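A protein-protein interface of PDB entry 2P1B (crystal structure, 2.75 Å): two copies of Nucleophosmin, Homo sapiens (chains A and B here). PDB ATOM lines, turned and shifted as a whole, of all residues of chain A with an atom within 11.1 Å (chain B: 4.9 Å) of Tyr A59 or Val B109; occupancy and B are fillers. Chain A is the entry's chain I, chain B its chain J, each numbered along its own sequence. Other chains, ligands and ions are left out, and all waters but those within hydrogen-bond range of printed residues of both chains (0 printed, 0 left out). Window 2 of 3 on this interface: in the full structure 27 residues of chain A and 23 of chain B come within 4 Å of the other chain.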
ATOM      1  N   GLN A  33      13.311  -4.102  41.585  1.00  0.00           N
ATOM      2  CA  GLN A  33      14.501  -3.782  40.772  1.00  0.00           C
ATOM      3  C   GLN A  33      15.817  -4.393  41.308  1.00  0.00           C
ATOM      4  O   GLN A  33      15.998  -4.554  42.524  1.00  0.00           O
ATOM      5  CB  GLN A  33      14.680  -2.264  40.660  1.00  0.00           C
ATOM      6  CG  GLN A  33      15.436  -1.812  39.430  1.00  0.00           C
ATOM      7  CD  GLN A  33      14.605  -2.005  38.158  1.00  0.00           C
ATOM      8  OE1 GLN A  33      15.042  -1.714  37.066  1.00  0.00           O
ATOM      9  NE2 GLN A  33      13.394  -2.502  38.309  1.00  0.00           N
ATOM     10  N   GLU A  55      21.798 -11.039  31.394  1.00  0.00           N
ATOM     11  CA  GLU A  55      20.657 -11.189  30.504  1.00  0.00           C
ATOM     12  C   GLU A  55      19.326 -10.862  31.175  1.00  0.00           C
ATOM     13  O   GLU A  55      18.822 -11.598  32.026  1.00  0.00           O
ATOM     14  CB  GLU A  55      20.619 -12.593  29.890  1.00  0.00           C
ATOM     15  CG  GLU A  55      19.960 -12.613  28.517  1.00  0.00           C
ATOM     16  CD  GLU A  55      19.971 -13.985  27.870  1.00  0.00           C
ATOM     17  OE1 GLU A  55      19.755 -14.981  28.592  1.00  0.00           O
ATOM     18  OE2 GLU A  55      20.180 -14.068  26.639  1.00  0.00           O
ATOM     19  N   ALA A  56      18.790  -9.716  30.772  1.00  0.00           N
ATOM     20  CA  ALA A  56      17.523  -9.192  31.239  1.00  0.00           C
ATOM     21  C   ALA A  56      16.971  -8.505  29.989  1.00  0.00           C
ATOM     22  O   ALA A  56      17.715  -8.262  29.037  1.00  0.00           O
ATOM     23  CB  ALA A  56      17.757  -8.197  32.348  1.00  0.00           C
ATOM     24  N   MET A  57      15.683  -8.190  29.980  1.00  0.00           N
ATOM     25  CA  MET A  57      15.074  -7.573  28.805  1.00  0.00           C
ATOM     26  C   MET A  57      15.460  -6.143  28.444  1.00  0.00           C
ATOM     27  O   MET A  57      15.788  -5.330  29.313  1.00  0.00           O
ATOM     28  CB  MET A  57      13.558  -7.672  28.919  1.00  0.00           C
ATOM     29  CG  MET A  57      12.948  -8.626  27.913  1.00  0.00           C
ATOM     30  SD  MET A  57      11.217  -8.888  28.243  1.00  0.00           S
ATOM     31  CE  MET A  57      10.626  -7.151  28.361  1.00  0.00           C
ATOM     32  N   ASN A  58      15.410  -5.850  27.144  1.00  0.00           N
ATOM     33  CA  ASN A  58      15.718  -4.517  26.635  1.00  0.00           C
ATOM     34  C   ASN A  58      14.412  -3.763  26.341  1.00  0.00           C
ATOM     35  O   ASN A  58      13.327  -4.351  26.351  1.00  0.00           O
ATOM     36  CB  ASN A  58      16.571  -4.612  25.372  1.00  0.00           C
ATOM     37  CG  ASN A  58      15.747  -4.786  24.130  1.00  0.00           C
ATOM     38  OD1 ASN A  58      14.978  -3.903  23.764  1.00  0.00           O
ATOM     39  ND2 ASN A  58      15.897  -5.924  23.470  1.00  0.00           N
ATOM     40  N   TYR A  59      14.521  -2.470  26.051  1.00  0.00           N
ATOM     41  CA  TYR A  59      13.344  -1.638  25.829  1.00  0.00           C
ATOM     42  C   TYR A  59      12.150  -2.204  25.068  1.00  0.00           C
ATOM     43  O   TYR A  59      11.006  -2.040  25.492  1.00  0.00           O
ATOM     44  CB  TYR A  59      13.729  -0.305  25.176  1.00  0.00           C
ATOM     45  CG  TYR A  59      12.537   0.624  25.043  1.00  0.00           C
ATOM     46  CD1 TYR A  59      11.692   0.850  26.132  1.00  0.00           C
ATOM     47  CD2 TYR A  59      12.226   1.241  23.831  1.00  0.00           C
ATOM     48  CE1 TYR A  59      10.565   1.659  26.023  1.00  0.00           C
ATOM     49  CE2 TYR A  59      11.098   2.056  23.708  1.00  0.00           C
ATOM     50  CZ  TYR A  59      10.271   2.260  24.808  1.00  0.00           C
ATOM     51  OH  TYR A  59       9.152   3.059  24.694  1.00  0.00           O
ATOM     52  N   GLU A  60      12.403  -2.869  23.952  1.00  0.00           N
ATOM     53  CA  GLU A  60      11.315  -3.380  23.129  1.00  0.00           C
ATOM     54  C   GLU A  60      10.560  -4.612  23.640  1.00  0.00           C
ATOM     55  O   GLU A  60       9.329  -4.623  23.652  1.00  0.00           O
ATOM     56  CB  GLU A  60      11.838  -3.618  21.705  1.00  0.00           C
ATOM     57  CG  GLU A  60      12.343  -2.341  21.003  1.00  0.00           C
ATOM     58  CD  GLU A  60      13.490  -1.639  21.744  1.00  0.00           C
ATOM     59  OE1 GLU A  60      14.510  -2.293  22.043  1.00  0.00           O
ATOM     60  OE2 GLU A  60      13.380  -0.425  22.019  1.00  0.00           O
ATOM     61  N   GLY A  61      11.287  -5.639  24.060  1.00  0.00           N
ATOM     62  CA  GLY A  61      10.642  -6.849  24.544  1.00  0.00           C
ATOM     63  C   GLY A  61      11.562  -8.043  24.401  1.00  0.00           C
ATOM     64  O   GLY A  61      11.455  -9.030  25.132  1.00  0.00           O
ATOM     65  N   SER A  62      12.469  -7.956  23.436  1.00  0.00           N
ATOM     66  CA  SER A  62      13.437  -9.012  23.206  1.00  0.00           C
ATOM     67  C   SER A  62      14.453  -8.977  24.347  1.00  0.00           C
ATOM     68  O   SER A  62      14.702  -7.926  24.939  1.00  0.00           O
ATOM     69  CB  SER A  62      14.134  -8.795  21.859  1.00  0.00           C
ATOM     70  OG  SER A  62      14.503  -7.435  21.685  1.00  0.00           O
ATOM     71  N   PRO A  63      15.038 -10.134  24.688  1.00  0.00           N
ATOM     72  CA  PRO A  63      16.021 -10.180  25.769  1.00  0.00           C
ATOM     73  C   PRO A  63      17.424  -9.944  25.218  1.00  0.00           C
ATOM     74  O   PRO A  63      17.747 -10.437  24.139  1.00  0.00           O
ATOM     75  CB  PRO A  63      15.851 -11.595  26.304  1.00  0.00           C
ATOM     76  CG  PRO A  63      15.672 -12.368  25.040  1.00  0.00           C
ATOM     77  CD  PRO A  63      14.711 -11.496  24.224  1.00  0.00           C
ATOM     78  N   ILE A  64      18.250  -9.181  25.933  1.00  0.00           N
ATOM     79  CA  ILE A  64      19.618  -8.962  25.466  1.00  0.00           C
ATOM     80  C   ILE A  64      20.647  -9.529  26.417  1.00  0.00           C
ATOM     81  O   ILE A  64      20.405  -9.669  27.616  1.00  0.00           O
ATOM     82  CB  ILE A  64      20.005  -7.471  25.281  1.00  0.00           C
ATOM     83  CG1 ILE A  64      19.381  -6.624  26.384  1.00  0.00           C
ATOM     84  CG2 ILE A  64      19.682  -7.015  23.872  1.00  0.00           C
ATOM     85  CD1 ILE A  64      19.974  -5.233  26.460  1.00  0.00           C
ATOM     86  N   LYS A  65      21.794  -9.867  25.839  1.00  0.00           N
ATOM     87  CA  LYS A  65      22.939 -10.368  26.578  1.00  0.00           C
ATOM     88  C   LYS A  65      23.862  -9.157  26.556  1.00  0.00           C
ATOM     89  O   LYS A  65      24.105  -8.558  25.503  1.00  0.00           O
ATOM     90  CB  LYS A  65      23.592 -11.555  25.868  1.00  0.00           C
ATOM     91  CG  LYS A  65      22.729 -12.803  25.801  1.00  0.00           C
ATOM     92  CD  LYS A  65      23.552 -13.976  25.310  1.00  0.00           C
ATOM     93  CE  LYS A  65      22.715 -14.995  24.551  1.00  0.00           C
ATOM     94  NZ  LYS A  65      23.558 -15.792  23.601  1.00  0.00           N
ATOM     95  N   VAL A  66      24.365  -8.799  27.726  1.00  0.00           N
ATOM     96  CA  VAL A  66      25.206  -7.627  27.865  1.00  0.00           C
ATOM     97  C   VAL A  66      26.416  -7.891  28.747  1.00  0.00           C
ATOM     98  O   VAL A  66      26.340  -8.691  29.666  1.00  0.00           O
ATOM     99  CB  VAL A  66      24.353  -6.497  28.464  1.00  0.00           C
ATOM    100  CG1 VAL A  66      25.188  -5.611  29.359  1.00  0.00           C
ATOM    101  CG2 VAL A  66      23.706  -5.708  27.344  1.00  0.00           C
ATOM    102  N   GLU A  85      21.188  -0.785  37.920  1.00  0.00           N
ATOM    103  CA  GLU A  85      19.870  -1.376  38.139  1.00  0.00           C
ATOM    104  C   GLU A  85      19.338  -2.046  36.869  1.00  0.00           C
ATOM    105  O   GLU A  85      19.322  -1.450  35.791  1.00  0.00           O
ATOM    106  CB  GLU A  85      18.883  -0.310  38.611  1.00  0.00           C
ATOM    107  CG  GLU A  85      18.988   0.073  40.084  1.00  0.00           C
ATOM    108  CD  GLU A  85      18.377   1.444  40.376  1.00  0.00           C
ATOM    109  OE1 GLU A  85      19.077   2.464  40.187  1.00  0.00           O
ATOM    110  OE2 GLU A  85      17.194   1.508  40.778  1.00  0.00           O
ATOM    111  N   ILE A  86      18.912  -3.296  37.010  1.00  0.00           N
ATOM    112  CA  ILE A  86      18.374  -4.072  35.899  1.00  0.00           C
ATOM    113  C   ILE A  86      17.021  -4.641  36.323  1.00  0.00           C
ATOM    114  O   ILE A  86      16.873  -5.138  37.449  1.00  0.00           O
ATOM    115  CB  ILE A  86      19.320  -5.225  35.522  1.00  0.00           C
ATOM    116  CG1 ILE A  86      20.729  -4.682  35.299  1.00  0.00           C
ATOM    117  CG2 ILE A  86      18.845  -5.892  34.255  1.00  0.00           C
ATOM    118  CD1 ILE A  86      21.699  -5.693  34.727  1.00  0.00           C
ATOM    119  N   THR A  87      16.042  -4.561  35.424  1.00  0.00           N
ATOM    120  CA  THR A  87      14.689  -5.037  35.702  1.00  0.00           C
ATOM    121  C   THR A  87      14.511  -6.548  35.500  1.00  0.00           C
ATOM    122  O   THR A  87      14.810  -7.094  34.434  1.00  0.00           O
ATOM    123  CB  THR A  87      13.669  -4.279  34.845  1.00  0.00           C
ATOM    124  OG1 THR A  87      13.885  -2.868  34.997  1.00  0.00           O
ATOM    125  CG2 THR A  87      12.251  -4.622  35.282  1.00  0.00           C
ATOM    126  N   GLN B   7      11.627   4.668  33.521  1.00  0.00           N
ATOM    127  CA  GLN B   7      11.663   3.187  33.317  1.00  0.00           C
ATOM    128  C   GLN B   7      12.945   2.731  32.616  1.00  0.00           C
ATOM    129  O   GLN B   7      13.443   3.401  31.711  1.00  0.00           O
ATOM    130  CB  GLN B   7      10.424   2.751  32.540  1.00  0.00           C
ATOM    131  CG  GLN B   7       9.154   3.207  33.226  1.00  0.00           C
ATOM    132  CD  GLN B   7       7.963   2.351  32.886  1.00  0.00           C
ATOM    133  OE1 GLN B   7       7.346   2.508  31.831  1.00  0.00           O
ATOM    134  NE2 GLN B   7       7.635   1.422  33.780  1.00  0.00           N
ATOM    135  N   TYR B   9      15.606  -0.472  30.908  1.00  0.00           N
ATOM    136  CA  TYR B   9      15.806  -1.740  30.241  1.00  0.00           C
ATOM    137  C   TYR B   9      17.302  -1.856  29.964  1.00  0.00           C
ATOM    138  O   TYR B   9      17.997  -0.843  29.831  1.00  0.00           O
ATOM    139  CB  TYR B   9      15.029  -1.757  28.924  1.00  0.00           C
ATOM    140  CG  TYR B   9      13.617  -1.246  29.055  1.00  0.00           C
ATOM    141  CD1 TYR B   9      13.360   0.120  29.156  1.00  0.00           C
ATOM    142  CD2 TYR B   9      12.536  -2.127  29.136  1.00  0.00           C
ATOM    143  CE1 TYR B   9      12.065   0.600  29.342  1.00  0.00           C
ATOM    144  CE2 TYR B   9      11.237  -1.655  29.323  1.00  0.00           C
ATOM    145  CZ  TYR B   9      11.010  -0.290  29.427  1.00  0.00           C
ATOM    146  OH  TYR B   9       9.737   0.190  29.638  1.00  0.00           O
ATOM    147  N   LEU B  10      17.806  -3.086  29.898  1.00  0.00           N
ATOM    148  CA  LEU B  10      19.217  -3.277  29.616  1.00  0.00           C
ATOM    149  C   LEU B  10      19.532  -2.748  28.241  1.00  0.00           C
ATOM    150  O   LEU B  10      18.667  -2.657  27.371  1.00  0.00           O
ATOM    151  CB  LEU B  10      19.606  -4.751  29.647  1.00  0.00           C
ATOM    152  CG  LEU B  10      20.192  -5.330  30.929  1.00  0.00           C
ATOM    153  CD1 LEU B  10      20.884  -6.637  30.596  1.00  0.00           C
ATOM    154  CD2 LEU B  10      21.189  -4.354  31.538  1.00  0.00           C
ATOM    155  N   GLU B  31      10.543  11.850  25.886  1.00  0.00           N
ATOM    156  CA  GLU B  31      11.608  11.772  26.876  1.00  0.00           C
ATOM    157  C   GLU B  31      12.362  10.462  26.703  1.00  0.00           C
ATOM    158  O   GLU B  31      11.751   9.400  26.594  1.00  0.00           O
ATOM    159  CB  GLU B  31      11.040  11.930  28.288  1.00  0.00           C
ATOM    160  CG  GLU B  31      10.325  13.250  28.525  1.00  0.00           C
ATOM    161  CD  GLU B  31       9.776  13.372  29.933  1.00  0.00           C
ATOM    162  OE1 GLU B  31       9.955  12.422  30.723  1.00  0.00           O
ATOM    163  OE2 GLU B  31       9.167  14.416  30.244  1.00  0.00           O
ATOM    164  N   HIS B  32      13.688  10.530  26.705  1.00  0.00           N
ATOM    165  CA  HIS B  32      14.491   9.326  26.507  1.00  0.00           C
ATOM    166  C   HIS B  32      15.964   9.576  26.761  1.00  0.00           C
ATOM    167  O   HIS B  32      16.515  10.579  26.325  1.00  0.00           O
ATOM    168  CB  HIS B  32      14.316   8.810  25.079  1.00  0.00           C
ATOM    169  CG  HIS B  32      13.507   7.561  24.979  1.00  0.00           C
ATOM    170  ND1 HIS B  32      13.918   6.358  25.518  1.00  0.00           N
ATOM    171  CD2 HIS B  32      12.312   7.320  24.396  1.00  0.00           C
ATOM    172  CE1 HIS B  32      13.008   5.439  25.271  1.00  0.00           C
ATOM    173  NE2 HIS B  32      12.021   5.995  24.589  1.00  0.00           N
ATOM    174  N   HIS B 107      18.660   1.848  29.135  1.00  0.00           N
ATOM    175  CA  HIS B 107      17.721   2.539  28.264  1.00  0.00           C
ATOM    176  C   HIS B 107      16.647   3.123  29.192  1.00  0.00           C
ATOM    177  O   HIS B 107      15.755   2.404  29.669  1.00  0.00           O
ATOM    178  CB  HIS B 107      17.104   1.525  27.296  1.00  0.00           C
ATOM    179  CG  HIS B 107      16.466   2.136  26.087  1.00  0.00           C
ATOM    180  ND1 HIS B 107      15.742   3.307  26.130  1.00  0.00           N
ATOM    181  CD2 HIS B 107      16.381   1.692  24.808  1.00  0.00           C
ATOM    182  CE1 HIS B 107      15.237   3.556  24.935  1.00  0.00           C
ATOM    183  NE2 HIS B 107      15.610   2.591  24.116  1.00  0.00           N
ATOM    184  N   LEU B 108      16.749   4.421  29.470  1.00  0.00           N
ATOM    185  CA  LEU B 108      15.791   5.087  30.346  1.00  0.00           C
ATOM    186  C   LEU B 108      14.693   5.735  29.511  1.00  0.00           C
ATOM    187  O   LEU B 108      14.980   6.360  28.490  1.00  0.00           O
ATOM    188  CB  LEU B 108      16.506   6.134  31.204  1.00  0.00           C
ATOM    189  CG  LEU B 108      17.630   5.624  32.118  1.00  0.00           C
ATOM    190  CD1 LEU B 108      18.263   6.816  32.817  1.00  0.00           C
ATOM    191  CD2 LEU B 108      17.097   4.618  33.138  1.00  0.00           C
ATOM    192  N   VAL B 109      13.446   5.590  29.966  1.00  0.00           N
ATOM    193  CA  VAL B 109      12.270   6.108  29.255  1.00  0.00           C
ATOM    194  C   VAL B 109      11.308   7.020  30.026  1.00  0.00           C
ATOM    195  O   VAL B 109      10.909   6.713  31.150  1.00  0.00           O
ATOM    196  CB  VAL B 109      11.394   4.955  28.727  1.00  0.00           C
ATOM    197  CG1 VAL B 109      10.437   5.475  27.671  1.00  0.00           C
ATOM    198  CG2 VAL B 109      12.256   3.838  28.187  1.00  0.00           C
ATOM    199  N   ALA B 110      10.918   8.114  29.366  1.00  0.00           N
ATOM    200  CA  ALA B 110       9.963   9.108  29.868  1.00  0.00           C
ATOM    201  C   ALA B 110       9.244   8.744  31.167  1.00  0.00           C
ATOM    202  O   ALA B 110       8.016   8.494  31.104  1.00  0.00           O
ATOM    203  CB  ALA B 110       8.927   9.394  28.776  1.00  0.00           C
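The backbone carbonyl oxygen (O) of Met A57 lies within hydrogen-bond range of the backbone NH (N) of Leu B10 (3.1 Å).
The side-chain amide oxygen (OD1) of Asn A58 lies close to the side-chain carboxylate (OE1) of Glu A60 (2.4 Å).
N of Ile A64 is in hydrogen-bond range of O of Ala A56, at 3.3 Å.
N of Val B109 lies within hydrogen-bond range of O of Gln B7 (2.8 Å).
The backbone carbonyl oxygen (O) of Tyr B9 is in hydrogen-bond range of the backbone NH (N) of His B107.
The side-chain hydroxyl (OG) of Ser A62 lies within hydrogen-bond range of the side-chain amide nitrogen (ND2) of Asn A58 (2.7 Å).
Hydrophobic or aromatic side chains of chain A within 4 Å of the printed part of chain B: Ala A56, Tyr A59, Ile A64 and Ile A86.
Among the printed residues, 10 pairs touch across the chains.
Among the printed residues, no Asp or Glu carboxylate lies within 4 Å of a Lys or Arg side-chain nitrogen of the other chain.
Among the printed residues, pairs that only touch across the chains: Tyr A59 with Tyr B9, Ile A64 with Leu B10, Asn A58 with Tyr B9, Tyr A59 with His B107, Asn A58 with Leu B10, Ile A86 with Leu B10, Tyr A59 with Val B109, Met A57 with Tyr B9 and Ala A56 with Leu B10.
Of the printed residues of chain B, Ala A56 touches Leu B10 (3.7 Å).
Printed residues of chain B within 4 Å of Asn A58: Tyr B9 and Leu B10.
Of chain B, only Tyr B9, His B107 and Val B109 come within 4 Å of Tyr A59.
Of the printed residues of chain B, Ile A64 touches Leu B10.
Of the printed residues of chain B, Ile A86 touches Leu B10.
No residue of chain A comes within 4 Å of Gln B7.
Of chain A, only Met A57, Asn A58 and Tyr A59 come within 4 Å of Tyr B9.
Printed residues of chain A within 4 Å of Leu B10: Ala A56 (3.7 Å), Met A57 (3.1 Å), Asn A58 (3.5 Å), Ile A64 (3.0 Å) and Ile A86 (3.5 Å).
No residue of chain A comes within 4 Å of His B32.
Of chain A, only Tyr A59 (3.3 Å) comes within 4 Å of His B107.
No residue of chain A comes within 4 Å of Leu B108.
Of chain A, only Tyr A59 comes within 4 Å of Val B109.
Ala B110 touches none of the printed residues of chain A.
The nearest residue of chain B that does not touch Tyr A59 is His B32 (4.1 Å).
The nearest residue of chain A that does not touch Val B109 is Glu A60 (7.6 Å).
No position is printed for both chains.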
